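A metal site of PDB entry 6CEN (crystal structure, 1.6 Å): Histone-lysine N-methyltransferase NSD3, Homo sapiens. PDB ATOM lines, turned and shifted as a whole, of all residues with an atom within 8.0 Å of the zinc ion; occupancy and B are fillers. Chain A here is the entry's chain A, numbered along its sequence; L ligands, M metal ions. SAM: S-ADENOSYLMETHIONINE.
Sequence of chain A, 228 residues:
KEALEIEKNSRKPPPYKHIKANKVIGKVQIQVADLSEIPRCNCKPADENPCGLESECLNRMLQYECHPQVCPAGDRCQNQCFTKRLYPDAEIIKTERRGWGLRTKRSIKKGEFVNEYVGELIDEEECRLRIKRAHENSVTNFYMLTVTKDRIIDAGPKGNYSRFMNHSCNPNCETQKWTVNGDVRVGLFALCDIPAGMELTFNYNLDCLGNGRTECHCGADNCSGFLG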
ATOM      1  N   ARG A  98      10.886   5.847  16.773  1.00  0.00           N
ATOM      2  CA  ARG A  98      10.876   7.299  16.910  1.00  0.00           C
ATOM      3  C   ARG A  98      11.068   7.692  18.387  1.00  0.00           C
ATOM      4  O   ARG A  98      10.726   8.782  18.800  1.00  0.00           O
ATOM      5  CB  ARG A  98       9.607   7.907  16.310  1.00  0.00           C
ATOM      6  CG  ARG A  98       9.466   7.627  14.809  1.00  0.00           C
ATOM      7  CD  ARG A  98       8.158   8.111  14.214  1.00  0.00           C
ATOM      8  NE  ARG A  98       7.061   7.331  14.756  1.00  0.00           N
ATOM      9  CZ  ARG A  98       6.191   7.721  15.677  1.00  0.00           C
ATOM     10  NH1 ARG A  98       6.126   8.995  16.049  1.00  0.00           N
ATOM     11  NH2 ARG A  98       5.315   6.856  16.183  1.00  0.00           N
ATOM     12  N   HIS A 167       8.172  14.366  14.855  1.00  0.00           N
ATOM     13  CA  HIS A 167       7.948  14.886  13.503  1.00  0.00           C
ATOM     14  C   HIS A 167       7.031  13.984  12.715  1.00  0.00           C
ATOM     15  O   HIS A 167       7.205  12.777  12.735  1.00  0.00           O
ATOM     16  CB  HIS A 167       9.267  14.996  12.726  1.00  0.00           C
ATOM     17  CG  HIS A 167       9.068  15.225  11.265  1.00  0.00           C
ATOM     18  ND1 HIS A 167       8.786  16.453  10.743  1.00  0.00           N
ATOM     19  CD2 HIS A 167       8.997  14.353  10.230  1.00  0.00           C
ATOM     20  CE1 HIS A 167       8.587  16.351   9.435  1.00  0.00           C
ATOM     21  NE2 HIS A 167       8.702  15.076   9.108  1.00  0.00           N
ATOM     22  N   SER A 168       6.082  14.581  11.998  1.00  0.00           N
ATOM     23  CA  SER A 168       5.385  13.865  10.946  1.00  0.00           C
ATOM     24  C   SER A 168       5.334  14.658   9.674  1.00  0.00           C
ATOM     25  O   SER A 168       5.174  15.878   9.686  1.00  0.00           O
ATOM     26  CB  SER A 168       3.950  13.508  11.384  1.00  0.00           C
ATOM     27  OG  SER A 168       3.257  12.805  10.334  1.00  0.00           O
ATOM     28  N   CYS A 169       5.439  13.955   8.549  1.00  0.00           N
ATOM     29  CA  CYS A 169       5.198  14.507   7.237  1.00  0.00           C
ATOM     30  C   CYS A 169       3.723  14.790   6.934  1.00  0.00           C
ATOM     31  O   CYS A 169       3.416  15.558   6.002  1.00  0.00           O
ATOM     32  CB  CYS A 169       5.791  13.545   6.186  1.00  0.00           C
ATOM     33  SG  CYS A 169       7.601  13.292   6.376  1.00  0.00           S
ATOM     34  N   ASN A 170       2.822  14.204   7.718  1.00  0.00           N
ATOM     35  CA  ASN A 170       1.387  14.460   7.651  1.00  0.00           C
ATOM     36  C   ASN A 170       0.899  14.682   9.063  1.00  0.00           C
ATOM     37  O   ASN A 170       0.241  13.844   9.636  1.00  0.00           O
ATOM     38  CB  ASN A 170       0.670  13.323   6.953  1.00  0.00           C
ATOM     39  CG  ASN A 170      -0.802  13.606   6.774  1.00  0.00           C
ATOM     40  OD1 ASN A 170      -1.181  14.736   6.530  1.00  0.00           O
ATOM     41  ND2 ASN A 170      -1.632  12.596   6.954  1.00  0.00           N
ATOM     42  N   GLU A 215      16.743   9.480   8.871  1.00  0.00           N
ATOM     43  CA  GLU A 215      15.610   8.764   8.308  1.00  0.00           C
ATOM     44  C   GLU A 215      14.316   9.089   9.075  1.00  0.00           C
ATOM     45  O   GLU A 215      14.320   9.178  10.299  1.00  0.00           O
ATOM     46  CB  GLU A 215      15.908   7.264   8.378  1.00  0.00           C
ATOM     47  CG  GLU A 215      14.865   6.312   7.817  1.00  0.00           C
ATOM     48  CD  GLU A 215      15.374   4.878   7.773  1.00  0.00           C
ATOM     49  OE1 GLU A 215      16.499   4.626   8.248  1.00  0.00           O
ATOM     50  OE2 GLU A 215      14.654   3.990   7.264  1.00  0.00           O
ATOM     51  N   CYS A 216      13.210   9.246   8.346  1.00  0.00           N
ATOM     52  CA  CYS A 216      11.906   9.499   8.960  1.00  0.00           C
ATOM     53  C   CYS A 216      11.091   8.213   9.017  1.00  0.00           C
ATOM     54  O   CYS A 216      10.981   7.515   8.006  1.00  0.00           O
ATOM     55  CB  CYS A 216      11.126  10.577   8.203  1.00  0.00           C
ATOM     56  SG  CYS A 216       9.564  11.023   8.994  1.00  0.00           S
ATOM     57  N   HIS A 217      10.507   7.933  10.177  1.00  0.00           N
ATOM     58  CA  HIS A 217       9.598   6.800  10.380  1.00  0.00           C
ATOM     59  C   HIS A 217       8.172   7.196  10.693  1.00  0.00           C
ATOM     60  O   HIS A 217       7.432   6.470  11.383  1.00  0.00           O
ATOM     61  CB  HIS A 217      10.173   5.834  11.426  1.00  0.00           C
ATOM     62  CG  HIS A 217      11.512   5.303  11.056  1.00  0.00           C
ATOM     63  ND1 HIS A 217      11.679   4.378  10.055  1.00  0.00           N
ATOM     64  CD2 HIS A 217      12.747   5.557  11.539  1.00  0.00           C
ATOM     65  CE1 HIS A 217      12.967   4.102   9.921  1.00  0.00           C
ATOM     66  NE2 HIS A 217      13.627   4.797  10.813  1.00  0.00           N
ATOM     67  N   CYS A 218       7.736   8.356  10.165  1.00  0.00           N
ATOM     68  CA  CYS A 218       6.414   8.850  10.528  1.00  0.00           C
ATOM     69  C   CYS A 218       5.274   7.995  10.007  1.00  0.00           C
ATOM     70  O   CYS A 218       4.186   8.007  10.563  1.00  0.00           O
ATOM     71  CB  CYS A 218       6.212  10.318  10.107  1.00  0.00           C
ATOM     72  SG  CYS A 218       5.892  10.598   8.341  1.00  0.00           S
ATOM     73  N   GLY A 219       5.518   7.276   8.927  1.00  0.00           N
ATOM     74  CA  GLY A 219       4.517   6.373   8.396  1.00  0.00           C
ATOM     75  C   GLY A 219       3.505   7.009   7.422  1.00  0.00           C
ATOM     76  O   GLY A 219       2.642   6.291   6.858  1.00  0.00           O
ATOM     77  N   ALA A 220       3.621   8.314   7.182  1.00  0.00           N
ATOM     78  CA  ALA A 220       2.665   9.009   6.303  1.00  0.00           C
ATOM     79  C   ALA A 220       2.776   8.561   4.840  1.00  0.00           C
ATOM     80  O   ALA A 220       3.862   8.257   4.381  1.00  0.00           O
ATOM     81  CB  ALA A 220       2.866  10.497   6.386  1.00  0.00           C
ATOM     82  N   ASP A 221       1.657   8.615   4.120  1.00  0.00           N
ATOM     83  CA  ASP A 221       1.669   8.298   2.673  1.00  0.00           C
ATOM     84  C   ASP A 221       2.617   9.224   1.900  1.00  0.00           C
ATOM     85  O   ASP A 221       3.211   8.824   0.900  1.00  0.00           O
ATOM     86  CB  ASP A 221       0.278   8.396   2.060  1.00  0.00           C
ATOM     87  CG  ASP A 221      -0.647   7.262   2.476  1.00  0.00           C
ATOM     88  OD1 ASP A 221      -0.242   6.352   3.217  1.00  0.00           O
ATOM     89  OD2 ASP A 221      -1.818   7.307   2.030  1.00  0.00           O
ATOM     90  N   ASN A 222       2.724  10.476   2.334  1.00  0.00           N
ATOM     91  CA  ASN A 222       3.586  11.462   1.687  1.00  0.00           C
ATOM     92  C   ASN A 222       4.940  11.630   2.374  1.00  0.00           C
ATOM     93  O   ASN A 222       5.631  12.613   2.114  1.00  0.00           O
ATOM     94  CB  ASN A 222       2.879  12.823   1.653  1.00  0.00           C
ATOM     95  CG  ASN A 222       2.678  13.392   3.034  1.00  0.00           C
ATOM     96  OD1 ASN A 222       2.096  12.731   3.887  1.00  0.00           O
ATOM     97  ND2 ASN A 222       3.113  14.604   3.247  1.00  0.00           N
ATOM     98  N   CYS A 223       5.357  10.674   3.222  1.00  0.00           N
ATOM     99  CA  CYS A 223       6.665  10.751   3.868  1.00  0.00           C
ATOM    100  C   CYS A 223       7.778  10.903   2.836  1.00  0.00           C
ATOM    101  O   CYS A 223       7.823  10.128   1.889  1.00  0.00           O
ATOM    102  CB  CYS A 223       6.949   9.508   4.671  1.00  0.00           C
ATOM    103  SG  CYS A 223       8.459   9.689   5.654  1.00  0.00           S
ATOM    104  N   SER A 224       8.661  11.868   3.017  1.00  0.00           N
ATOM    105  CA  SER A 224       9.783  12.096   2.105  1.00  0.00           C
ATOM    106  C   SER A 224      10.837  11.023   2.279  1.00  0.00           C
ATOM    107  O   SER A 224      11.678  10.841   1.389  1.00  0.00           O
ATOM    108  CB  SER A 224      10.434  13.440   2.336  1.00  0.00           C
ATOM    109  OG  SER A 224      11.128  13.449   3.569  1.00  0.00           O
ATOM    110  N   GLY A 225      10.822  10.389   3.458  1.00  0.00           N
ATOM    111  CA  GLY A 225      11.829   9.416   3.878  1.00  0.00           C
ATOM    112  C   GLY A 225      12.841  10.049   4.816  1.00  0.00           C
ATOM    113  O   GLY A 225      13.649   9.337   5.416  1.00  0.00           O
ATOM    114  N   PHE A 226      12.803  11.366   4.971  1.00  0.00           N
ATOM    115  CA  PHE A 226      13.802  12.047   5.723  1.00  0.00           C
ATOM    116  C   PHE A 226      13.209  13.039   6.635  1.00  0.00           C
ATOM    117  O   PHE A 226      12.190  13.695   6.356  1.00  0.00           O
ATOM    118  CB  PHE A 226      14.838  12.742   4.840  1.00  0.00           C
ATOM    119  CG  PHE A 226      15.429  11.837   3.841  1.00  0.00           C
ATOM    120  CD1 PHE A 226      16.404  10.927   4.226  1.00  0.00           C
ATOM    121  CD2 PHE A 226      15.008  11.881   2.520  1.00  0.00           C
ATOM    122  CE1 PHE A 226      16.955  10.069   3.293  1.00  0.00           C
ATOM    123  CE2 PHE A 226      15.559  11.023   1.587  1.00  0.00           C
ATOM    124  CZ  PHE A 226      16.547  10.114   1.978  1.00  0.00           C
ATOM    125  N   LEU A 227      13.896  13.147   7.751  1.00  0.00           N
ATOM    126  CA  LEU A 227      13.361  13.802   8.879  1.00  0.00           C
ATOM    127  C   LEU A 227      13.329  15.296   8.639  1.00  0.00           C
ATOM    128  O   LEU A 227      14.259  15.868   8.032  1.00  0.00           O
ATOM    129  CB  LEU A 227      14.185  13.429  10.110  1.00  0.00           C
ATOM    130  CG  LEU A 227      13.614  13.863  11.429  1.00  0.00           C
ATOM    131  CD1 LEU A 227      12.330  13.119  11.693  1.00  0.00           C
ATOM    132  CD2 LEU A 227      14.650  13.604  12.514  1.00  0.00           C
ATOM    133  N   GLY A 228      12.223  15.898   9.046  1.00  0.00           N
ATOM    134  CA  GLY A 228      12.071  17.346   9.054  1.00  0.00           C
ATOM    135  C   GLY A 228      11.525  17.918   7.776  1.00  0.00           C
ATOM    136  O   GLY A 228      11.350  17.206   6.790  1.00  0.00           O
ATOM    137  OXT GLY A 228      11.273  19.137   7.716  1.00  0.00           O
HETATM  138  N   SAM L   1      11.516  11.057  20.120  1.00  0.00           N
HETATM  139  CA  SAM L   1      12.159  12.097  20.939  1.00  0.00           C
HETATM  140  C   SAM L   1      12.669  11.491  22.235  1.00  0.00           C
HETATM  141  O   SAM L   1      13.063  12.234  23.184  1.00  0.00           O
HETATM  142  OXT SAM L   1      12.684  10.236  22.303  1.00  0.00           O
HETATM  143  CB  SAM L   1      11.187  13.263  21.153  1.00  0.00           C
HETATM  144  CG  SAM L   1      11.215  14.307  20.032  1.00  0.00           C
HETATM  145  SD  SAM L   1      12.662  15.158  19.872  1.00  0.00           S
HETATM  146  CE  SAM L   1      12.235  16.757  19.858  1.00  0.00           C
HETATM  147  C5' SAM L   1      13.193  14.952  18.285  1.00  0.00           C
HETATM  148  C4' SAM L   1      13.999  13.707  17.930  1.00  0.00           C
HETATM  149  O4' SAM L   1      13.164  12.564  17.867  1.00  0.00           O
HETATM  150  C3' SAM L   1      14.644  13.810  16.552  1.00  0.00           C
HETATM  151  O3' SAM L   1      15.912  14.470  16.625  1.00  0.00           O
HETATM  152  C2' SAM L   1      14.726  12.366  16.133  1.00  0.00           C
HETATM  153  O2' SAM L   1      15.872  11.769  16.736  1.00  0.00           O
HETATM  154  C1' SAM L   1      13.465  11.753  16.734  1.00  0.00           C
HETATM  155  N9  SAM L   1      12.331  11.791  15.789  1.00  0.00           N
HETATM  156  C8  SAM L   1      11.283  12.640  15.820  1.00  0.00           C
HETATM  157  N7  SAM L   1      10.404  12.427  14.818  1.00  0.00           N
HETATM  158  C5  SAM L   1      10.910  11.351  14.162  1.00  0.00           C
HETATM  159  C6  SAM L   1      10.499  10.626  12.963  1.00  0.00           C
HETATM  160  N6  SAM L   1       9.370  10.953  12.375  1.00  0.00           N
HETATM  161  N1  SAM L   1      11.296   9.628  12.549  1.00  0.00           N
HETATM  162  C2  SAM L   1      12.451   9.311  13.162  1.00  0.00           C
HETATM  163  N3  SAM L   1      12.909   9.936  14.264  1.00  0.00           N
HETATM  164  C4  SAM L   1      12.171  10.978  14.755  1.00  0.00           C
HETATM  165 ZN    ZN M   1       7.932  11.186   7.335  1.00  0.00          ZN
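N of His 167 sits at hydrogen-bond distance from N7 of the ligand (3.0 Å).
A nitrogen (N) of the ligand is in hydrogen-bond range of the backbone carbonyl oxygen of Arg 98 (2.7 Å).
N1 of the ligand is in hydrogen-bond range of N of His 217.
SG of Cys 216 sits close to N6 of the ligand (3.4 Å).
The backbone carbonyl oxygen (O) of His 167 lies within hydrogen-bond range of a nitrogen (N6) of the ligand, 2.9 Å away.
The side-chain sulfur (SG) of Cys 218 lies close to the backbone NH (N) of Ala 220, 3.4 Å away.
The backbone NH (N) of Cys 169 lies within hydrogen-bond range of a ring nitrogen (NE2) of His 167 (3.5 Å).
N of Cys 216 sits at hydrogen-bond distance from O of Gly 225.
O of Cys 169 is in hydrogen-bond range of ND2 of Asn 222.
The side-chain sulfur of Cys 169 lies close to the backbone NH of Ser 224 (3.8 Å).
N of Gly 225 lies close to SG of Cys 223 (3.3 Å).
Within 4 Å of the zinc ion: Cys 169, Cys 216, Cys 218 and Cys 223.
Along chain A the residues within 4 Å of the zinc ion span positions 169 to 223.
The nearest printed residue that does not touch the zinc ion is His 167 (4.3 Å).
SG of Cys 223 is bound to the zinc ion, at 2.3 Å.
SG of Cys 216 binds the zinc ion.
The zinc ion is bound by SG of Cys 169 (2.3 Å).
The zinc ion is bound by the side-chain sulfur (SG) of Cys 218, at 2.3 Å.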
